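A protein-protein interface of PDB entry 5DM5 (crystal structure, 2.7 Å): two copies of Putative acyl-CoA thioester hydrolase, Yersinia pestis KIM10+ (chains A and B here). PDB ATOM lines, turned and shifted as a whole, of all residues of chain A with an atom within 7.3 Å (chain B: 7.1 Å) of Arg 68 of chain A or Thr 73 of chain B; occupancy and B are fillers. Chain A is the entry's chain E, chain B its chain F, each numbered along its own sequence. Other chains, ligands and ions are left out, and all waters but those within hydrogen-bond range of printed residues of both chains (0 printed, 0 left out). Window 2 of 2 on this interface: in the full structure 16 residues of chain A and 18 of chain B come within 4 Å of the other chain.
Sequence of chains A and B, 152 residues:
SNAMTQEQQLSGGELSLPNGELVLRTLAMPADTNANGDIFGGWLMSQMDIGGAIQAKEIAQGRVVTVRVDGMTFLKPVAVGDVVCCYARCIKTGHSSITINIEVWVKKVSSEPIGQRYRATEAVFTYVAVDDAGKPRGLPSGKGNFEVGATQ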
ATOM      1  N   VAL A  65     -13.549  15.232 -32.795  1.00  0.00           N
ATOM      2  CA  VAL A  65     -14.563  14.195 -32.989  1.00  0.00           C
ATOM      3  C   VAL A  65     -14.325  13.049 -32.016  1.00  0.00           C
ATOM      4  O   VAL A  65     -13.194  12.594 -31.856  1.00  0.00           O
ATOM      5  CB  VAL A  65     -14.565  13.632 -34.436  1.00  0.00           C
ATOM      6  CG1 VAL A  65     -15.375  12.345 -34.522  1.00  0.00           C
ATOM      7  CG2 VAL A  65     -15.096  14.660 -35.420  1.00  0.00           C
ATOM      8  N   THR A  66     -15.389  12.608 -31.351  1.00  0.00           N
ATOM      9  CA  THR A  66     -15.315  11.475 -30.444  1.00  0.00           C
ATOM     10  C   THR A  66     -15.143  10.165 -31.239  1.00  0.00           C
ATOM     11  O   THR A  66     -15.842   9.915 -32.225  1.00  0.00           O
ATOM     12  CB  THR A  66     -16.563  11.425 -29.520  1.00  0.00           C
ATOM     13  OG1 THR A  66     -16.827  12.738 -29.003  1.00  0.00           O
ATOM     14  CG2 THR A  66     -16.354  10.472 -28.345  1.00  0.00           C
ATOM     15  N   VAL A  67     -14.159   9.368 -30.825  1.00  0.00           N
ATOM     16  CA  VAL A  67     -13.831   8.103 -31.477  1.00  0.00           C
ATOM     17  C   VAL A  67     -13.743   6.917 -30.515  1.00  0.00           C
ATOM     18  O   VAL A  67     -13.797   5.769 -30.953  1.00  0.00           O
ATOM     19  CB  VAL A  67     -12.521   8.213 -32.252  1.00  0.00           C
ATOM     20  CG1 VAL A  67     -12.692   9.176 -33.428  1.00  0.00           C
ATOM     21  CG2 VAL A  67     -11.396   8.646 -31.327  1.00  0.00           C
ATOM     22  N   ARG A  68     -13.530   7.176 -29.225  1.00  0.00           N
ATOM     23  CA  ARG A  68     -13.457   6.067 -28.271  1.00  0.00           C
ATOM     24  C   ARG A  68     -13.807   6.437 -26.831  1.00  0.00           C
ATOM     25  O   ARG A  68     -13.629   7.566 -26.420  1.00  0.00           O
ATOM     26  CB  ARG A  68     -12.082   5.413 -28.334  1.00  0.00           C
ATOM     27  CG  ARG A  68     -11.970   4.212 -27.452  1.00  0.00           C
ATOM     28  CD  ARG A  68     -10.689   3.464 -27.671  1.00  0.00           C
ATOM     29  NE  ARG A  68     -10.692   2.225 -26.893  1.00  0.00           N
ATOM     30  CZ  ARG A  68     -11.192   1.061 -27.294  1.00  0.00           C
ATOM     31  NH1 ARG A  68     -11.743   0.944 -28.493  1.00  0.00           N
ATOM     32  NH2 ARG A  68     -11.133   0.008 -26.487  1.00  0.00           N
ATOM     33  N   VAL A  69     -14.385   5.495 -26.095  1.00  0.00           N
ATOM     34  CA  VAL A  69     -14.648   5.665 -24.666  1.00  0.00           C
ATOM     35  C   VAL A  69     -14.184   4.444 -23.887  1.00  0.00           C
ATOM     36  O   VAL A  69     -14.677   3.352 -24.078  1.00  0.00           O
ATOM     37  CB  VAL A  69     -16.132   5.904 -24.359  1.00  0.00           C
ATOM     38  CG1 VAL A  69     -16.355   5.927 -22.873  1.00  0.00           C
ATOM     39  CG2 VAL A  69     -16.607   7.188 -24.996  1.00  0.00           C
ATOM     40  N   ASP A  70     -13.254   4.642 -22.974  1.00  0.00           N
ATOM     41  CA  ASP A  70     -12.656   3.522 -22.270  1.00  0.00           C
ATOM     42  C   ASP A  70     -13.028   3.582 -20.795  1.00  0.00           C
ATOM     43  O   ASP A  70     -13.172   4.659 -20.222  1.00  0.00           O
ATOM     44  CB  ASP A  70     -11.124   3.553 -22.402  1.00  0.00           C
ATOM     45  CG  ASP A  70     -10.643   4.203 -23.705  1.00  0.00           C
ATOM     46  OD1 ASP A  70     -10.184   3.450 -24.590  1.00  0.00           O
ATOM     47  OD2 ASP A  70     -10.721   5.453 -23.850  1.00  0.00           O
ATOM     48  N   GLY A  71     -13.214   2.421 -20.192  1.00  0.00           N
ATOM     49  CA  GLY A  71     -13.370   2.336 -18.758  1.00  0.00           C
ATOM     50  C   GLY A  71     -14.409   3.255 -18.171  1.00  0.00           C
ATOM     51  O   GLY A  71     -14.145   3.922 -17.193  1.00  0.00           O
ATOM     52  N   ILE A  98      -6.267  12.385 -28.763  1.00  0.00           N
ATOM     53  CA  ILE A  98      -6.310  13.153 -27.519  1.00  0.00           C
ATOM     54  C   ILE A  98      -7.151  12.405 -26.489  1.00  0.00           C
ATOM     55  O   ILE A  98      -8.367  12.381 -26.586  1.00  0.00           O
ATOM     56  CB  ILE A  98      -6.937  14.556 -27.708  1.00  0.00           C
ATOM     57  CG1 ILE A  98      -6.275  15.316 -28.852  1.00  0.00           C
ATOM     58  CG2 ILE A  98      -6.873  15.357 -26.409  1.00  0.00           C
ATOM     59  CD1 ILE A  98      -6.908  16.673 -29.110  1.00  0.00           C
ATOM     60  N   VAL A 124     -12.787   7.384 -19.229  1.00  0.00           N
ATOM     61  CA  VAL A 124     -11.657   7.937 -19.979  1.00  0.00           C
ATOM     62  C   VAL A 124     -11.954   8.084 -21.479  1.00  0.00           C
ATOM     63  O   VAL A 124     -11.914   7.114 -22.222  1.00  0.00           O
ATOM     64  CB  VAL A 124     -10.414   7.085 -19.833  1.00  0.00           C
ATOM     65  CG1 VAL A 124      -9.275   7.745 -20.580  1.00  0.00           C
ATOM     66  CG2 VAL A 124     -10.052   6.926 -18.380  1.00  0.00           C
ATOM     67  N   PHE A 125     -12.177   9.310 -21.930  1.00  0.00           N
ATOM     68  CA  PHE A 125     -12.586   9.581 -23.308  1.00  0.00           C
ATOM     69  C   PHE A 125     -11.440   9.761 -24.265  1.00  0.00           C
ATOM     70  O   PHE A 125     -10.425  10.285 -23.900  1.00  0.00           O
ATOM     71  CB  PHE A 125     -13.428  10.848 -23.382  1.00  0.00           C
ATOM     72  CG  PHE A 125     -14.855  10.649 -23.011  1.00  0.00           C
ATOM     73  CD1 PHE A 125     -15.219  10.418 -21.711  1.00  0.00           C
ATOM     74  CD2 PHE A 125     -15.827  10.622 -23.986  1.00  0.00           C
ATOM     75  CE1 PHE A 125     -16.533  10.226 -21.379  1.00  0.00           C
ATOM     76  CE2 PHE A 125     -17.138  10.424 -23.663  1.00  0.00           C
ATOM     77  CZ  PHE A 125     -17.495  10.225 -22.359  1.00  0.00           C
ATOM     78  N   THR A 126     -11.595   9.318 -25.497  1.00  0.00           N
ATOM     79  CA  THR A 126     -10.540   9.492 -26.485  1.00  0.00           C
ATOM     80  C   THR A 126     -11.119  10.163 -27.744  1.00  0.00           C
ATOM     81  O   THR A 126     -12.044   9.628 -28.387  1.00  0.00           O
ATOM     82  CB  THR A 126      -9.846   8.141 -26.829  1.00  0.00           C
ATOM     83  OG1 THR A 126      -9.368   7.518 -25.627  1.00  0.00           O
ATOM     84  CG2 THR A 126      -8.670   8.367 -27.764  1.00  0.00           C
ATOM     85  N   TYR A 127     -10.559  11.337 -28.064  1.00  0.00           N
ATOM     86  CA  TYR A 127     -10.956  12.218 -29.172  1.00  0.00           C
ATOM     87  C   TYR A 127      -9.912  12.294 -30.290  1.00  0.00           C
ATOM     88  O   TYR A 127      -8.768  11.883 -30.111  1.00  0.00           O
ATOM     89  CB  TYR A 127     -11.244  13.646 -28.657  1.00  0.00           C
ATOM     90  CG  TYR A 127     -12.436  13.772 -27.735  1.00  0.00           C
ATOM     91  CD1 TYR A 127     -13.676  14.139 -28.245  1.00  0.00           C
ATOM     92  CD2 TYR A 127     -12.340  13.531 -26.372  1.00  0.00           C
ATOM     93  CE1 TYR A 127     -14.797  14.255 -27.425  1.00  0.00           C
ATOM     94  CE2 TYR A 127     -13.461  13.644 -25.542  1.00  0.00           C
ATOM     95  CZ  TYR A 127     -14.687  14.006 -26.081  1.00  0.00           C
ATOM     96  OH  TYR A 127     -15.809  14.132 -25.294  1.00  0.00           O
ATOM     97  N   VAL A 128     -10.328  12.821 -31.441  1.00  0.00           N
ATOM     98  CA  VAL A 128      -9.458  13.008 -32.602  1.00  0.00           C
ATOM     99  C   VAL A 128      -9.694  14.379 -33.246  1.00  0.00           C
ATOM    100  O   VAL A 128     -10.824  14.702 -33.590  1.00  0.00           O
ATOM    101  CB  VAL A 128      -9.688  11.904 -33.657  1.00  0.00           C
ATOM    102  CG1 VAL A 128      -8.984  12.241 -34.951  1.00  0.00           C
ATOM    103  CG2 VAL A 128      -9.197  10.579 -33.146  1.00  0.00           C
ATOM    104  N   MET B  48     -27.422   3.084 -27.260  1.00  0.00           N
ATOM    105  CA  MET B  48     -26.740   1.857 -26.924  1.00  0.00           C
ATOM    106  C   MET B  48     -27.148   1.459 -25.547  1.00  0.00           C
ATOM    107  O   MET B  48     -27.421   0.303 -25.275  1.00  0.00           O
ATOM    108  CB  MET B  48     -25.243   2.071 -27.018  1.00  0.00           C
ATOM    109  CG  MET B  48     -24.848   2.597 -28.383  1.00  0.00           C
ATOM    110  SD  MET B  48     -23.108   2.913 -28.625  1.00  0.00           S
ATOM    111  CE  MET B  48     -22.591   1.207 -28.460  1.00  0.00           C
ATOM    112  N   ASP B  70     -17.313  -0.234 -21.480  1.00  0.00           N
ATOM    113  CA  ASP B  70     -15.906  -0.478 -21.729  1.00  0.00           C
ATOM    114  C   ASP B  70     -15.698  -0.497 -23.216  1.00  0.00           C
ATOM    115  O   ASP B  70     -16.604  -0.844 -23.950  1.00  0.00           O
ATOM    116  CB  ASP B  70     -15.463  -1.803 -21.119  1.00  0.00           C
ATOM    117  CG  ASP B  70     -15.437  -1.773 -19.611  1.00  0.00           C
ATOM    118  OD1 ASP B  70     -14.853  -0.842 -19.021  1.00  0.00           O
ATOM    119  OD2 ASP B  70     -16.035  -2.678 -19.004  1.00  0.00           O
ATOM    120  N   GLY B  71     -14.542  -0.052 -23.671  1.00  0.00           N
ATOM    121  CA  GLY B  71     -14.155  -0.233 -25.058  1.00  0.00           C
ATOM    122  C   GLY B  71     -15.128   0.160 -26.163  1.00  0.00           C
ATOM    123  O   GLY B  71     -15.278  -0.580 -27.132  1.00  0.00           O
ATOM    124  N   MET B  72     -15.758   1.329 -26.053  1.00  0.00           N
ATOM    125  CA  MET B  72     -16.634   1.803 -27.115  1.00  0.00           C
ATOM    126  C   MET B  72     -15.839   2.450 -28.234  1.00  0.00           C
ATOM    127  O   MET B  72     -15.078   3.371 -27.989  1.00  0.00           O
ATOM    128  CB  MET B  72     -17.651   2.810 -26.599  1.00  0.00           C
ATOM    129  CG  MET B  72     -18.558   3.316 -27.723  1.00  0.00           C
ATOM    130  SD  MET B  72     -20.082   4.099 -27.193  1.00  0.00           S
ATOM    131  CE  MET B  72     -19.329   5.334 -26.184  1.00  0.00           C
ATOM    132  N   THR B  73     -16.088   2.034 -29.471  1.00  0.00           N
ATOM    133  CA  THR B  73     -15.345   2.528 -30.630  1.00  0.00           C
ATOM    134  C   THR B  73     -16.264   3.144 -31.674  1.00  0.00           C
ATOM    135  O   THR B  73     -17.188   2.489 -32.149  1.00  0.00           O
ATOM    136  CB  THR B  73     -14.570   1.392 -31.346  1.00  0.00           C
ATOM    137  OG1 THR B  73     -13.840   0.599 -30.399  1.00  0.00           O
ATOM    138  CG2 THR B  73     -13.622   1.971 -32.390  1.00  0.00           C
ATOM    139  N   PHE B  74     -15.976   4.375 -32.082  1.00  0.00           N
ATOM    140  CA  PHE B  74     -16.748   5.024 -33.140  1.00  0.00           C
ATOM    141  C   PHE B  74     -16.087   4.789 -34.503  1.00  0.00           C
ATOM    142  O   PHE B  74     -15.274   5.593 -34.946  1.00  0.00           O
ATOM    143  CB  PHE B  74     -16.875   6.529 -32.866  1.00  0.00           C
ATOM    144  CG  PHE B  74     -17.636   6.872 -31.604  1.00  0.00           C
ATOM    145  CD1 PHE B  74     -18.935   7.326 -31.664  1.00  0.00           C
ATOM    146  CD2 PHE B  74     -17.043   6.761 -30.362  1.00  0.00           C
ATOM    147  CE1 PHE B  74     -19.619   7.650 -30.512  1.00  0.00           C
ATOM    148  CE2 PHE B  74     -17.726   7.083 -29.214  1.00  0.00           C
ATOM    149  CZ  PHE B  74     -19.010   7.526 -29.289  1.00  0.00           C
ATOM    150  N   LEU B  75     -16.489   3.716 -35.181  1.00  0.00           N
ATOM    151  CA  LEU B  75     -15.833   3.270 -36.412  1.00  0.00           C
ATOM    152  C   LEU B  75     -16.059   4.270 -37.534  1.00  0.00           C
ATOM    153  O   LEU B  75     -15.121   4.800 -38.120  1.00  0.00           O
ATOM    154  CB  LEU B  75     -16.353   1.889 -36.833  1.00  0.00           C
ATOM    155  CG  LEU B  75     -16.155   0.663 -35.924  1.00  0.00           C
ATOM    156  CD1 LEU B  75     -14.724   0.533 -35.454  1.00  0.00           C
ATOM    157  CD2 LEU B  75     -17.113   0.635 -34.748  1.00  0.00           C
ATOM    158  N   LYS B  76     -17.319   4.499 -37.857  1.00  0.00           N
ATOM    159  CA  LYS B  76     -17.646   5.478 -38.871  1.00  0.00           C
ATOM    160  C   LYS B  76     -18.732   6.400 -38.332  1.00  0.00           C
ATOM    161  O   LYS B  76     -19.610   5.974 -37.570  1.00  0.00           O
ATOM    162  CB  LYS B  76     -18.066   4.836 -40.195  1.00  0.00           C
ATOM    163  CG  LYS B  76     -17.003   3.962 -40.846  1.00  0.00           C
ATOM    164  CD  LYS B  76     -17.317   3.819 -42.337  1.00  0.00           C
ATOM    165  CE  LYS B  76     -16.712   2.583 -42.991  1.00  0.00           C
ATOM    166  NZ  LYS B  76     -17.324   2.332 -44.335  1.00  0.00           N
ATOM    167  N   ARG B 119     -20.800  -1.176 -40.066  1.00  0.00           N
ATOM    168  CA  ARG B 119     -20.808  -1.061 -38.598  1.00  0.00           C
ATOM    169  C   ARG B 119     -20.347   0.300 -38.108  1.00  0.00           C
ATOM    170  O   ARG B 119     -19.274   0.777 -38.487  1.00  0.00           O
ATOM    171  CB  ARG B 119     -19.911  -2.115 -37.947  1.00  0.00           C
ATOM    172  CG  ARG B 119     -19.971  -2.106 -36.413  1.00  0.00           C
ATOM    173  CD  ARG B 119     -19.066  -3.166 -35.782  1.00  0.00           C
ATOM    174  NE  ARG B 119     -17.662  -2.979 -36.150  1.00  0.00           N
ATOM    175  CZ  ARG B 119     -16.660  -3.749 -35.735  1.00  0.00           C
ATOM    176  NH1 ARG B 119     -16.888  -4.774 -34.926  1.00  0.00           N
ATOM    177  NH2 ARG B 119     -15.419  -3.488 -36.129  1.00  0.00           N
ATOM    178  N   ALA B 120     -21.169   0.915 -37.261  1.00  0.00           N
ATOM    179  CA  ALA B 120     -20.904   2.259 -36.773  1.00  0.00           C
ATOM    180  C   ALA B 120     -20.415   2.277 -35.316  1.00  0.00           C
ATOM    181  O   ALA B 120     -19.743   3.235 -34.910  1.00  0.00           O
ATOM    182  CB  ALA B 120     -22.139   3.114 -36.921  1.00  0.00           C
ATOM    183  N   THR B 121     -20.736   1.248 -34.523  1.00  0.00           N
ATOM    184  CA  THR B 121     -20.242   1.251 -33.133  1.00  0.00           C
ATOM    185  C   THR B 121     -19.971  -0.148 -32.529  1.00  0.00           C
ATOM    186  O   THR B 121     -20.653  -1.117 -32.831  1.00  0.00           O
ATOM    187  CB  THR B 121     -21.207   2.006 -32.197  1.00  0.00           C
ATOM    188  OG1 THR B 121     -21.482   3.302 -32.726  1.00  0.00           O
ATOM    189  CG2 THR B 121     -20.592   2.184 -30.858  1.00  0.00           C
ATOM    190  N   GLU B 122     -18.976  -0.219 -31.647  1.00  0.00           N
ATOM    191  CA  GLU B 122     -18.592  -1.433 -30.942  1.00  0.00           C
ATOM    192  C   GLU B 122     -18.442  -1.070 -29.474  1.00  0.00           C
ATOM    193  O   GLU B 122     -17.792  -0.079 -29.169  1.00  0.00           O
ATOM    194  CB  GLU B 122     -17.249  -1.941 -31.482  1.00  0.00           C
ATOM    195  CG  GLU B 122     -16.613  -3.112 -30.745  1.00  0.00           C
ATOM    196  CD  GLU B 122     -15.217  -3.431 -31.265  1.00  0.00           C
ATOM    197  OE1 GLU B 122     -14.666  -2.609 -32.026  1.00  0.00           O
ATOM    198  OE2 GLU B 122     -14.674  -4.501 -30.921  1.00  0.00           O
ATOM    199  N   ALA B 123     -19.020  -1.848 -28.562  1.00  0.00           N
ATOM    200  CA  ALA B 123     -18.852  -1.532 -27.142  1.00  0.00           C
ATOM    201  C   ALA B 123     -19.174  -2.688 -26.204  1.00  0.00           C
ATOM    202  O   ALA B 123     -19.852  -3.631 -26.589  1.00  0.00           O
ATOM    203  CB  ALA B 123     -19.701  -0.340 -26.788  1.00  0.00           C
ATOM    204  N   VAL B 124     -18.707  -2.611 -24.965  1.00  0.00           N
ATOM    205  CA  VAL B 124     -19.068  -3.627 -23.990  1.00  0.00           C
ATOM    206  C   VAL B 124     -19.802  -2.999 -22.825  1.00  0.00           C
ATOM    207  O   VAL B 124     -19.199  -2.409 -21.932  1.00  0.00           O
ATOM    208  CB  VAL B 124     -17.846  -4.389 -23.462  1.00  0.00           C
ATOM    209  CG1 VAL B 124     -18.272  -5.381 -22.396  1.00  0.00           C
ATOM    210  CG2 VAL B 124     -17.119  -5.080 -24.606  1.00  0.00           C
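The guanidinium group of Arg 68 of chain A sits at hydrogen-bond distance from the side-chain hydroxyl of Thr 73 of chain B (2.9 Å).
The backbone carbonyl oxygen (O) of Val 69 of chain A is in hydrogen-bond range of the backbone NH (N) of Gly 71 of chain B, at 3.4 Å.
N of Val 69 of chain A sits at hydrogen-bond distance from O of Met 72 of chain B (2.9 Å).
The backbone NH (N) of Phe 74 of chain B lies within hydrogen-bond range of the backbone carbonyl oxygen (O) of Val 67 of chain A (2.8 Å).
The backbone carbonyl oxygen (O) of Val 124 of chain B sits at hydrogen-bond distance from the backbone NH (N) of Asp 70 of chain B (2.9 Å).
The backbone NH (N) of Thr 126 of chain A sits at hydrogen-bond distance from the backbone carbonyl oxygen (O) of Arg 68 of chain A, at 2.8 Å.
The backbone NH (N) of Thr 73 of chain B lies within hydrogen-bond range of the backbone carbonyl oxygen (O) of Glu 122 of chain B (2.7 Å).
NE of Arg 68 of chain A is in salt-bridge range of OD1 of Asp 70 of chain A, at 2.7 Å.
The backbone carbonyl oxygen of Thr 126 of chain A lies close to the backbone NH of Val 67 of chain A.
Gly 71 of chain A touches Asp 70 of chain B, but with the chains exchanged Asp 70 of chain A does not touch Gly 71 of chain B (4.3 Å).
3 positions are printed for both chains.
Of the 13 printed residues of chain A, 5 touch a printed residue of chain B.
Hydrophobic or aromatic side chains of chain A that line the printed part of chain B: Val 69.
Of the 14 printed residues of chain B, 5 touch a printed residue of chain A.
Hydrophobic or aromatic side chains of chain B that line the printed part of chain A: Met 72 and Phe 74.
Among the printed residues, 10 pairs touch across the chains.
Among the printed residues, no Asp or Glu carboxylate lies within 4 Å of a Lys or Arg side-chain nitrogen of the other chain.
Printed residues of chain B within 4 Å of Arg 68 of chain A: Gly 71, Met 72, Thr 73 and Phe 74.
Thr 73 of chain B touches just these residues of chain A: Val 67 (3.6 Å) and Arg 68 (2.9 Å).
Printed residues of chain A within 4 Å of Gly 71 of chain B: Arg 68 and Val 69.
Of the printed residues of chain B, Thr 66 of chain A touches Phe 74.
Printed residues of chain A within 4 Å of Phe 74 of chain B: Thr 66 (3.6 Å), Val 67 (2.8 Å) and Arg 68 (3.7 Å).
Printed residues of chain A within 4 Å of Met 72 of chain B: Arg 68 and Val 69.
The nearest residue of chain B that does not touch Arg 68 of chain A is Asp 70 of chain B (5.6 Å).
The nearest residue of chain A that does not touch Thr 73 of chain B is Val 69 of chain A (5.1 Å).
The nearest printed residue of chain B that does not touch Val 69 of chain A is Asp 70 of chain B (4.1 Å).
Among the printed residues, pairs that only touch across the chains: Thr 66 of chain A with Phe 74 of chain B, Val 67 of chain A with Thr 73 of chain B, Arg 68 of chain A with Gly 71 of chain B, Arg 68 of chain A with Met 72 of chain B, Arg 68 of chain A with Phe 74 of chain B and Gly 71 of chain A with Asp 70 of chain B.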
